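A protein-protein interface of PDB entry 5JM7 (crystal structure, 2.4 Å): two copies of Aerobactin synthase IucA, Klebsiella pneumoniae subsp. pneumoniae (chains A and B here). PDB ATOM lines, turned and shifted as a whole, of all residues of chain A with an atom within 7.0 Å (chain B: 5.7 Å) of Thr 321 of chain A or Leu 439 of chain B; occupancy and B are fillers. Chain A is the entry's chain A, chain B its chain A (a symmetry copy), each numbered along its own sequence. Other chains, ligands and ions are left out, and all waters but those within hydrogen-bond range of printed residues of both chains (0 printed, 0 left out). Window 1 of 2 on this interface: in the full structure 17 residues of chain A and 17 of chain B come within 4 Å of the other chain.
The guanidinium group (NH2) of Arg 323 of chain A is in hydrogen-bond range of the backbone carbonyl oxygen (O) of Arg 389 of chain B (3.2 Å).
O of Gln 434 of chain A lies within hydrogen-bond range of N of Val 441 of chain A (2.8 Å).
N of Gln 434 of chain A is in hydrogen-bond range of O of Gly 442 of chain A (2.9 Å).
OE1 of Gln 316 of chain A lies within hydrogen-bond range of NH1 of Arg 323 of chain A (3.4 Å).
The backbone NH (N) of Arg 323 of chain A sits at hydrogen-bond distance from the backbone carbonyl oxygen (O) of Leu 443 of chain A, 2.9 Å away.
O of Thr 321 of chain A lies within hydrogen-bond range of N of Leu 443 of chain A.
OE1 of Gln 408 of chain A lies close to O of Val 441 of chain A (3.1 Å).
Among the printed residues, merely in contact across the chains: Pro 320 of chain A with Leu 439 of chain B (3.8 Å), Thr 321 of chain A with Leu 439 of chain B (3.5 Å), Gln 434 of chain A with Leu 436 of chain B (3.3 Å) and Val 441 of chain A with Leu 436 of chain B (3.6 Å).
Leu 439 of chain B touches two residues of chain A.
Of the printed residues of chain B, Gln 434 of chain A touches Leu 436.
Printed residues of chain A within 4 Å of Arg 389 of chain B: Arg 323.
Of the printed residues of chain A, Leu 436 of chain B touches Gln 434 (3.3 Å) and Val 441 (3.6 Å).
Printed residues of chain B within 4 Å of Pro 320 of chain A: Leu 439.
Of the printed residues of chain B, Val 441 of chain A touches Leu 436.
Gln 408 of chain A touches none of the printed residues of chain B.
The nearest residue of chain B that does not touch Thr 321 of chain A is Val 441 of chain B (5.2 Å).
Printed residues of chain B that touch a printed residue of chain A: Arg 389, Leu 436 and Leu 439.
Along chain B the printed residues that touch a printed residue of chain A span positions 389 to 439.
Among the printed residues, no Asp or Glu carboxylate lies within 4 Å of a Lys or Arg side-chain nitrogen of the other chain.
2 positions are printed for both chains.
Of the 5 pairs that touch across the chains among the printed residues, none has its exchanged pair printed and touching as well.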
ATOM      1  N   GLN A 316      -5.216 -32.671   5.357  1.00  0.00           N
ATOM      2  CA  GLN A 316      -5.129 -31.237   5.135  1.00  0.00           C
ATOM      3  C   GLN A 316      -3.678 -30.795   5.103  1.00  0.00           C
ATOM      4  O   GLN A 316      -3.292 -29.984   4.256  1.00  0.00           O
ATOM      5  CB  GLN A 316      -5.907 -30.477   6.217  1.00  0.00           C
ATOM      6  CG  GLN A 316      -5.859 -28.964   6.014  1.00  0.00           C
ATOM      7  CD  GLN A 316      -6.655 -28.505   4.810  1.00  0.00           C
ATOM      8  OE1 GLN A 316      -7.894 -28.495   4.824  1.00  0.00           O
ATOM      9  NE2 GLN A 316      -5.948 -28.251   3.712  1.00  0.00           N
ATOM     10  N   ARG A 318      -1.144 -32.445   4.135  1.00  0.00           N
ATOM     11  CA  ARG A 318      -0.539 -32.912   2.890  1.00  0.00           C
ATOM     12  C   ARG A 318      -0.966 -32.065   1.690  1.00  0.00           C
ATOM     13  O   ARG A 318      -0.200 -31.922   0.734  1.00  0.00           O
ATOM     14  CB  ARG A 318      -0.905 -34.384   2.668  1.00  0.00           C
ATOM     15  CG  ARG A 318      -0.319 -35.025   1.440  1.00  0.00           C
ATOM     16  CD  ARG A 318      -0.758 -36.493   1.316  1.00  0.00           C
ATOM     17  NE  ARG A 318      -0.237 -37.120   0.105  1.00  0.00           N
ATOM     18  CZ  ARG A 318      -0.422 -38.393  -0.212  1.00  0.00           C
ATOM     19  NH1 ARG A 318      -1.138 -39.181   0.576  1.00  0.00           N
ATOM     20  NH2 ARG A 318       0.059 -38.864  -1.350  1.00  0.00           N
ATOM     21  N   PHE A 319      -2.170 -31.499   1.711  1.00  0.00           N
ATOM     22  CA  PHE A 319      -2.674 -30.676   0.607  1.00  0.00           C
ATOM     23  C   PHE A 319      -3.149 -29.331   1.140  1.00  0.00           C
ATOM     24  O   PHE A 319      -4.353 -29.051   1.174  1.00  0.00           O
ATOM     25  CB  PHE A 319      -3.798 -31.386  -0.148  1.00  0.00           C
ATOM     26  CG  PHE A 319      -3.362 -32.674  -0.788  1.00  0.00           C
ATOM     27  CD1 PHE A 319      -2.654 -32.667  -1.983  1.00  0.00           C
ATOM     28  CD2 PHE A 319      -3.689 -33.894  -0.211  1.00  0.00           C
ATOM     29  CE1 PHE A 319      -2.244 -33.866  -2.576  1.00  0.00           C
ATOM     30  CE2 PHE A 319      -3.291 -35.088  -0.805  1.00  0.00           C
ATOM     31  CZ  PHE A 319      -2.565 -35.072  -1.984  1.00  0.00           C
ATOM     32  N   PRO A 320      -2.222 -28.470   1.555  1.00  0.00           N
ATOM     33  CA  PRO A 320      -2.639 -27.202   2.188  1.00  0.00           C
ATOM     34  C   PRO A 320      -3.450 -26.288   1.274  1.00  0.00           C
ATOM     35  O   PRO A 320      -4.261 -25.497   1.774  1.00  0.00           O
ATOM     36  CB  PRO A 320      -1.307 -26.564   2.613  1.00  0.00           C
ATOM     37  CG  PRO A 320      -0.283 -27.177   1.665  1.00  0.00           C
ATOM     38  CD  PRO A 320      -0.756 -28.624   1.511  1.00  0.00           C
ATOM     39  N   THR A 321      -3.281 -26.383  -0.044  1.00  0.00           N
ATOM     40  CA  THR A 321      -4.057 -25.586  -0.989  1.00  0.00           C
ATOM     41  C   THR A 321      -5.420 -26.195  -1.275  1.00  0.00           C
ATOM     42  O   THR A 321      -6.146 -25.647  -2.106  1.00  0.00           O
ATOM     43  CB  THR A 321      -3.313 -25.450  -2.333  1.00  0.00           C
ATOM     44  OG1 THR A 321      -3.216 -26.751  -2.950  1.00  0.00           O
ATOM     45  CG2 THR A 321      -1.892 -24.921  -2.137  1.00  0.00           C
ATOM     46  N   PHE A 322      -5.753 -27.343  -0.679  1.00  0.00           N
ATOM     47  CA  PHE A 322      -7.045 -27.994  -0.874  1.00  0.00           C
ATOM     48  C   PHE A 322      -7.938 -27.811   0.347  1.00  0.00           C
ATOM     49  O   PHE A 322      -7.565 -28.200   1.459  1.00  0.00           O
ATOM     50  CB  PHE A 322      -6.863 -29.476  -1.206  1.00  0.00           C
ATOM     51  CG  PHE A 322      -8.120 -30.273  -1.116  1.00  0.00           C
ATOM     52  CD1 PHE A 322      -9.190 -30.003  -1.940  1.00  0.00           C
ATOM     53  CD2 PHE A 322      -8.172 -31.401  -0.316  1.00  0.00           C
ATOM     54  CE1 PHE A 322     -10.359 -30.759  -1.873  1.00  0.00           C
ATOM     55  CE2 PHE A 322      -9.327 -32.195  -0.273  1.00  0.00           C
ATOM     56  CZ  PHE A 322     -10.423 -31.869  -1.050  1.00  0.00           C
ATOM     57  N   ARG A 323      -9.135 -27.276   0.127  1.00  0.00           N
ATOM     58  CA  ARG A 323     -10.052 -26.933   1.207  1.00  0.00           C
ATOM     59  C   ARG A 323     -11.447 -27.445   0.883  1.00  0.00           C
ATOM     60  O   ARG A 323     -11.877 -27.424  -0.275  1.00  0.00           O
ATOM     61  CB  ARG A 323     -10.106 -25.398   1.441  1.00  0.00           C
ATOM     62  CG  ARG A 323      -8.785 -24.800   1.900  1.00  0.00           C
ATOM     63  CD  ARG A 323      -8.541 -25.135   3.355  1.00  0.00           C
ATOM     64  NE  ARG A 323      -9.205 -24.172   4.233  1.00  0.00           N
ATOM     65  CZ  ARG A 323      -9.599 -24.438   5.471  1.00  0.00           C
ATOM     66  NH1 ARG A 323      -9.414 -25.654   5.981  1.00  0.00           N
ATOM     67  NH2 ARG A 323     -10.183 -23.485   6.188  1.00  0.00           N
ATOM     68  N   HIS A 407      -2.634 -30.704 -10.854  1.00  0.00           N
ATOM     69  CA  HIS A 407      -1.957 -30.754  -9.565  1.00  0.00           C
ATOM     70  C   HIS A 407      -2.813 -30.162  -8.446  1.00  0.00           C
ATOM     71  O   HIS A 407      -2.712 -30.612  -7.296  1.00  0.00           O
ATOM     72  CB  HIS A 407      -0.604 -30.053  -9.674  1.00  0.00           C
ATOM     73  CG  HIS A 407       0.391 -30.810 -10.498  1.00  0.00           C
ATOM     74  ND1 HIS A 407       1.076 -30.244 -11.553  1.00  0.00           N
ATOM     75  CD2 HIS A 407       0.797 -32.102 -10.435  1.00  0.00           C
ATOM     76  CE1 HIS A 407       1.869 -31.147 -12.096  1.00  0.00           C
ATOM     77  NE2 HIS A 407       1.720 -32.282 -11.434  1.00  0.00           N
ATOM     78  N   GLN A 408      -3.676 -29.181  -8.755  1.00  0.00           N
ATOM     79  CA  GLN A 408      -4.478 -28.529  -7.720  1.00  0.00           C
ATOM     80  C   GLN A 408      -5.851 -29.152  -7.544  1.00  0.00           C
ATOM     81  O   GLN A 408      -6.375 -29.149  -6.427  1.00  0.00           O
ATOM     82  CB  GLN A 408      -4.686 -27.046  -8.026  1.00  0.00           C
ATOM     83  CG  GLN A 408      -3.442 -26.173  -8.029  1.00  0.00           C
ATOM     84  CD  GLN A 408      -2.661 -26.254  -6.716  1.00  0.00           C
ATOM     85  OE1 GLN A 408      -3.221 -26.467  -5.649  1.00  0.00           O
ATOM     86  NE2 GLN A 408      -1.357 -25.994  -6.796  1.00  0.00           N
ATOM     87  N   PRO A 412      -5.572 -33.849  -5.398  1.00  0.00           N
ATOM     88  CA  PRO A 412      -6.184 -34.014  -4.065  1.00  0.00           C
ATOM     89  C   PRO A 412      -7.390 -34.932  -4.068  1.00  0.00           C
ATOM     90  O   PRO A 412      -7.599 -35.668  -3.091  1.00  0.00           O
ATOM     91  CB  PRO A 412      -6.614 -32.587  -3.690  1.00  0.00           C
ATOM     92  CG  PRO A 412      -5.788 -31.681  -4.559  1.00  0.00           C
ATOM     93  CD  PRO A 412      -5.619 -32.436  -5.835  1.00  0.00           C
ATOM     94  N   GLN A 434      -9.273 -22.027  -7.210  1.00  0.00           N
ATOM     95  CA  GLN A 434      -8.648 -20.857  -6.611  1.00  0.00           C
ATOM     96  C   GLN A 434      -7.521 -20.444  -7.552  1.00  0.00           C
ATOM     97  O   GLN A 434      -6.536 -21.185  -7.708  1.00  0.00           O
ATOM     98  CB  GLN A 434      -8.073 -21.169  -5.233  1.00  0.00           C
ATOM     99  CG  GLN A 434      -7.680 -19.921  -4.409  1.00  0.00           C
ATOM    100  CD  GLN A 434      -6.942 -20.278  -3.114  1.00  0.00           C
ATOM    101  OE1 GLN A 434      -6.587 -21.450  -2.873  1.00  0.00           O
ATOM    102  NE2 GLN A 434      -6.781 -19.290  -2.242  1.00  0.00           N
ATOM    103  N   VAL A 441      -3.969 -22.102  -8.233  1.00  0.00           N
ATOM    104  CA  VAL A 441      -3.076 -22.319  -7.100  1.00  0.00           C
ATOM    105  C   VAL A 441      -3.734 -23.104  -5.970  1.00  0.00           C
ATOM    106  O   VAL A 441      -3.059 -23.420  -4.978  1.00  0.00           O
ATOM    107  CB  VAL A 441      -2.520 -20.987  -6.560  1.00  0.00           C
ATOM    108  CG1 VAL A 441      -1.645 -20.299  -7.602  1.00  0.00           C
ATOM    109  CG2 VAL A 441      -3.659 -20.086  -6.113  1.00  0.00           C
ATOM    110  N   GLY A 442      -5.019 -23.436  -6.089  1.00  0.00           N
ATOM    111  CA  GLY A 442      -5.689 -24.172  -5.032  1.00  0.00           C
ATOM    112  C   GLY A 442      -7.054 -24.652  -5.477  1.00  0.00           C
ATOM    113  O   GLY A 442      -7.583 -24.256  -6.527  1.00  0.00           O
ATOM    114  N   LEU A 443      -7.636 -25.487  -4.626  1.00  0.00           N
ATOM    115  CA  LEU A 443      -8.967 -26.029  -4.831  1.00  0.00           C
ATOM    116  C   LEU A 443      -9.823 -25.799  -3.593  1.00  0.00           C
ATOM    117  O   LEU A 443      -9.376 -26.022  -2.463  1.00  0.00           O
ATOM    118  CB  LEU A 443      -8.911 -27.546  -5.123  1.00  0.00           C
ATOM    119  CG  LEU A 443     -10.271 -28.251  -5.181  1.00  0.00           C
ATOM    120  CD1 LEU A 443     -11.136 -27.763  -6.363  1.00  0.00           C
ATOM    121  CD2 LEU A 443     -10.118 -29.765  -5.202  1.00  0.00           C
ATOM    122  N   ILE A 444     -11.070 -25.400  -3.802  1.00  0.00           N
ATOM    123  CA  ILE A 444     -12.077 -25.427  -2.746  1.00  0.00           C
ATOM    124  C   ILE A 444     -13.232 -26.287  -3.243  1.00  0.00           C
ATOM    125  O   ILE A 444     -13.794 -26.023  -4.317  1.00  0.00           O
ATOM    126  CB  ILE A 444     -12.558 -24.021  -2.361  1.00  0.00           C
ATOM    127  CG1 ILE A 444     -11.413 -23.212  -1.745  1.00  0.00           C
ATOM    128  CG2 ILE A 444     -13.683 -24.114  -1.349  1.00  0.00           C
ATOM    129  CD1 ILE A 444     -11.714 -21.744  -1.561  1.00  0.00           C
ATOM    130  N   GLN B 360       0.699 -10.703  -0.724  1.00  0.00           N
ATOM    131  CA  GLN B 360       1.586 -11.164   0.350  1.00  0.00           C
ATOM    132  C   GLN B 360       2.873 -11.714  -0.277  1.00  0.00           C
ATOM    133  O   GLN B 360       3.172 -12.911  -0.238  1.00  0.00           O
ATOM    134  CB  GLN B 360       0.923 -12.219   1.222  1.00  0.00           C
ATOM    135  CG  GLN B 360       1.751 -12.495   2.503  1.00  0.00           C
ATOM    136  CD  GLN B 360       1.180 -13.621   3.372  1.00  0.00           C
ATOM    137  OE1 GLN B 360       0.189 -14.249   3.016  1.00  0.00           O
ATOM    138  NE2 GLN B 360       1.790 -13.857   4.520  1.00  0.00           N
ATOM    139  N   LEU B 386      -0.919 -20.037   9.351  1.00  0.00           N
ATOM    140  CA  LEU B 386      -1.216 -21.145   8.446  1.00  0.00           C
ATOM    141  C   LEU B 386      -1.820 -22.314   9.227  1.00  0.00           C
ATOM    142  O   LEU B 386      -2.883 -22.839   8.877  1.00  0.00           O
ATOM    143  CB  LEU B 386       0.064 -21.578   7.703  1.00  0.00           C
ATOM    144  CG  LEU B 386      -0.064 -22.726   6.700  1.00  0.00           C
ATOM    145  CD1 LEU B 386      -0.998 -22.336   5.560  1.00  0.00           C
ATOM    146  CD2 LEU B 386       1.282 -23.169   6.151  1.00  0.00           C
ATOM    147  N   ARG B 389      -5.514 -21.338  10.307  1.00  0.00           N
ATOM    148  CA  ARG B 389      -6.501 -21.280   9.229  1.00  0.00           C
ATOM    149  C   ARG B 389      -6.863 -22.680   8.728  1.00  0.00           C
ATOM    150  O   ARG B 389      -8.034 -22.963   8.448  1.00  0.00           O
ATOM    151  CB  ARG B 389      -5.966 -20.399   8.097  1.00  0.00           C
ATOM    152  CG  ARG B 389      -6.876 -20.274   6.877  1.00  0.00           C
ATOM    153  CD  ARG B 389      -6.328 -19.297   5.833  1.00  0.00           C
ATOM    154  NE  ARG B 389      -5.060 -19.717   5.241  1.00  0.00           N
ATOM    155  CZ  ARG B 389      -4.948 -20.581   4.233  1.00  0.00           C
ATOM    156  NH1 ARG B 389      -6.032 -21.135   3.714  1.00  0.00           N
ATOM    157  NH2 ARG B 389      -3.755 -20.901   3.748  1.00  0.00           N
ATOM    158  N   ALA B 400       4.515 -28.000   5.745  1.00  0.00           N
ATOM    159  CA  ALA B 400       3.870 -27.548   4.517  1.00  0.00           C
ATOM    160  C   ALA B 400       4.582 -26.334   3.925  1.00  0.00           C
ATOM    161  O   ALA B 400       4.679 -26.208   2.698  1.00  0.00           O
ATOM    162  CB  ALA B 400       2.406 -27.232   4.779  1.00  0.00           C
ATOM    163  N   TRP B 401       5.106 -25.443   4.778  1.00  0.00           N
ATOM    164  CA  TRP B 401       5.730 -24.218   4.289  1.00  0.00           C
ATOM    165  C   TRP B 401       7.119 -24.518   3.728  1.00  0.00           C
ATOM    166  O   TRP B 401       7.518 -23.943   2.707  1.00  0.00           O
ATOM    167  CB  TRP B 401       5.851 -23.200   5.418  1.00  0.00           C
ATOM    168  CG  TRP B 401       5.997 -21.740   5.009  1.00  0.00           C
ATOM    169  CD1 TRP B 401       4.986 -20.809   5.008  1.00  0.00           C
ATOM    170  CD2 TRP B 401       7.153 -21.078   4.458  1.00  0.00           C
ATOM    171  NE1 TRP B 401       5.460 -19.595   4.584  1.00  0.00           N
ATOM    172  CE2 TRP B 401       6.780 -19.728   4.224  1.00  0.00           C
ATOM    173  CE3 TRP B 401       8.477 -21.478   4.182  1.00  0.00           C
ATOM    174  CZ2 TRP B 401       7.672 -18.777   3.711  1.00  0.00           C
ATOM    175  CZ3 TRP B 401       9.363 -20.535   3.669  1.00  0.00           C
ATOM    176  CH2 TRP B 401       8.952 -19.186   3.445  1.00  0.00           C
ATOM    177  N   ALA B 404       6.564 -26.287   0.271  1.00  0.00           N
ATOM    178  CA  ALA B 404       6.179 -25.365  -0.794  1.00  0.00           C
ATOM    179  C   ALA B 404       7.334 -24.433  -1.151  1.00  0.00           C
ATOM    180  O   ALA B 404       7.552 -24.126  -2.330  1.00  0.00           O
ATOM    181  CB  ALA B 404       4.946 -24.573  -0.380  1.00  0.00           C
ATOM    182  N   GLN B 434       6.262 -15.272  -2.864  1.00  0.00           N
ATOM    183  CA  GLN B 434       4.875 -14.911  -3.122  1.00  0.00           C
ATOM    184  C   GLN B 434       4.023 -15.875  -2.303  1.00  0.00           C
ATOM    185  O   GLN B 434       4.008 -17.085  -2.583  1.00  0.00           O
ATOM    186  CB  GLN B 434       4.523 -15.046  -4.600  1.00  0.00           C
ATOM    187  CG  GLN B 434       3.182 -14.388  -4.998  1.00  0.00           C
ATOM    188  CD  GLN B 434       2.778 -14.701  -6.442  1.00  0.00           C
ATOM    189  OE1 GLN B 434       3.415 -15.526  -7.129  1.00  0.00           O
ATOM    190  NE2 GLN B 434       1.771 -13.990  -6.935  1.00  0.00           N
ATOM    191  N   MET B 435       3.316 -15.365  -1.305  1.00  0.00           N
ATOM    192  CA  MET B 435       2.462 -16.203  -0.485  1.00  0.00           C
ATOM    193  C   MET B 435       0.987 -15.901  -0.741  1.00  0.00           C
ATOM    194  O   MET B 435       0.604 -14.784  -1.128  1.00  0.00           O
ATOM    195  CB  MET B 435       2.790 -16.018   0.997  1.00  0.00           C
ATOM    196  CG  MET B 435       4.127 -16.585   1.362  1.00  0.00           C
ATOM    197  SD  MET B 435       4.529 -16.356   3.088  1.00  0.00           S
ATOM    198  CE  MET B 435       5.083 -14.635   3.095  1.00  0.00           C
ATOM    199  N   LEU B 436       0.160 -16.921  -0.513  1.00  0.00           N
ATOM    200  CA  LEU B 436      -1.291 -16.801  -0.517  1.00  0.00           C
ATOM    201  C   LEU B 436      -1.770 -17.483   0.765  1.00  0.00           C
ATOM    202  O   LEU B 436      -1.626 -18.697   0.928  1.00  0.00           O
ATOM    203  CB  LEU B 436      -1.900 -17.436  -1.780  1.00  0.00           C
ATOM    204  CG  LEU B 436      -3.415 -17.236  -1.964  1.00  0.00           C
ATOM    205  CD1 LEU B 436      -3.734 -15.709  -2.069  1.00  0.00           C
ATOM    206  CD2 LEU B 436      -3.963 -17.953  -3.195  1.00  0.00           C
ATOM    207  N   GLY B 437      -2.330 -16.708   1.683  1.00  0.00           N
ATOM    208  CA  GLY B 437      -2.696 -17.263   2.972  1.00  0.00           C
ATOM    209  C   GLY B 437      -1.532 -17.884   3.711  1.00  0.00           C
ATOM    210  O   GLY B 437      -1.674 -18.979   4.285  1.00  0.00           O
ATOM    211  N   ASP B 438      -0.376 -17.215   3.702  1.00  0.00           N
ATOM    212  CA  ASP B 438       0.808 -17.621   4.456  1.00  0.00           C
ATOM    213  C   ASP B 438       1.505 -18.843   3.873  1.00  0.00           C
ATOM    214  O   ASP B 438       2.482 -19.323   4.458  1.00  0.00           O
ATOM    215  CB  ASP B 438       0.434 -17.850   5.920  1.00  0.00           C
ATOM    216  CG  ASP B 438       0.068 -16.546   6.627  1.00  0.00           C
ATOM    217  OD1 ASP B 438       0.627 -15.470   6.304  1.00  0.00           O
ATOM    218  OD2 ASP B 438      -0.927 -16.572   7.381  1.00  0.00           O
ATOM    219  N   LEU B 439       1.052 -19.362   2.728  1.00  0.00           N
ATOM    220  CA  LEU B 439       1.740 -20.481   2.078  1.00  0.00           C
ATOM    221  C   LEU B 439       2.434 -20.005   0.802  1.00  0.00           C
ATOM    222  O   LEU B 439       1.818 -19.268   0.019  1.00  0.00           O
ATOM    223  CB  LEU B 439       0.744 -21.579   1.688  1.00  0.00           C
ATOM    224  CG  LEU B 439       1.290 -22.858   1.063  1.00  0.00           C
ATOM    225  CD1 LEU B 439       1.947 -23.713   2.140  1.00  0.00           C
ATOM    226  CD2 LEU B 439       0.183 -23.605   0.375  1.00  0.00           C
ATOM    227  N   PRO B 440       3.689 -20.389   0.554  1.00  0.00           N
ATOM    228  CA  PRO B 440       4.339 -20.018  -0.720  1.00  0.00           C
ATOM    229  C   PRO B 440       3.590 -20.602  -1.915  1.00  0.00           C
ATOM    230  O   PRO B 440       3.365 -21.818  -1.998  1.00  0.00           O
ATOM    231  CB  PRO B 440       5.743 -20.627  -0.589  1.00  0.00           C
ATOM    232  CG  PRO B 440       6.003 -20.660   0.891  1.00  0.00           C
ATOM    233  CD  PRO B 440       4.641 -20.979   1.511  1.00  0.00           C
ATOM    234  N   VAL B 441       3.213 -19.731  -2.854  1.00  0.00           N
ATOM    235  CA  VAL B 441       2.633 -20.143  -4.128  1.00  0.00           C
ATOM    236  C   VAL B 441       3.449 -19.676  -5.328  1.00  0.00           C
ATOM    237  O   VAL B 441       3.103 -20.023  -6.469  1.00  0.00           O
ATOM    238  CB  VAL B 441       1.175 -19.663  -4.263  1.00  0.00           C
ATOM    239  CG1 VAL B 441       0.285 -20.319  -3.214  1.00  0.00           C
ATOM    240  CG2 VAL B 441       1.113 -18.147  -4.170  1.00  0.00           C
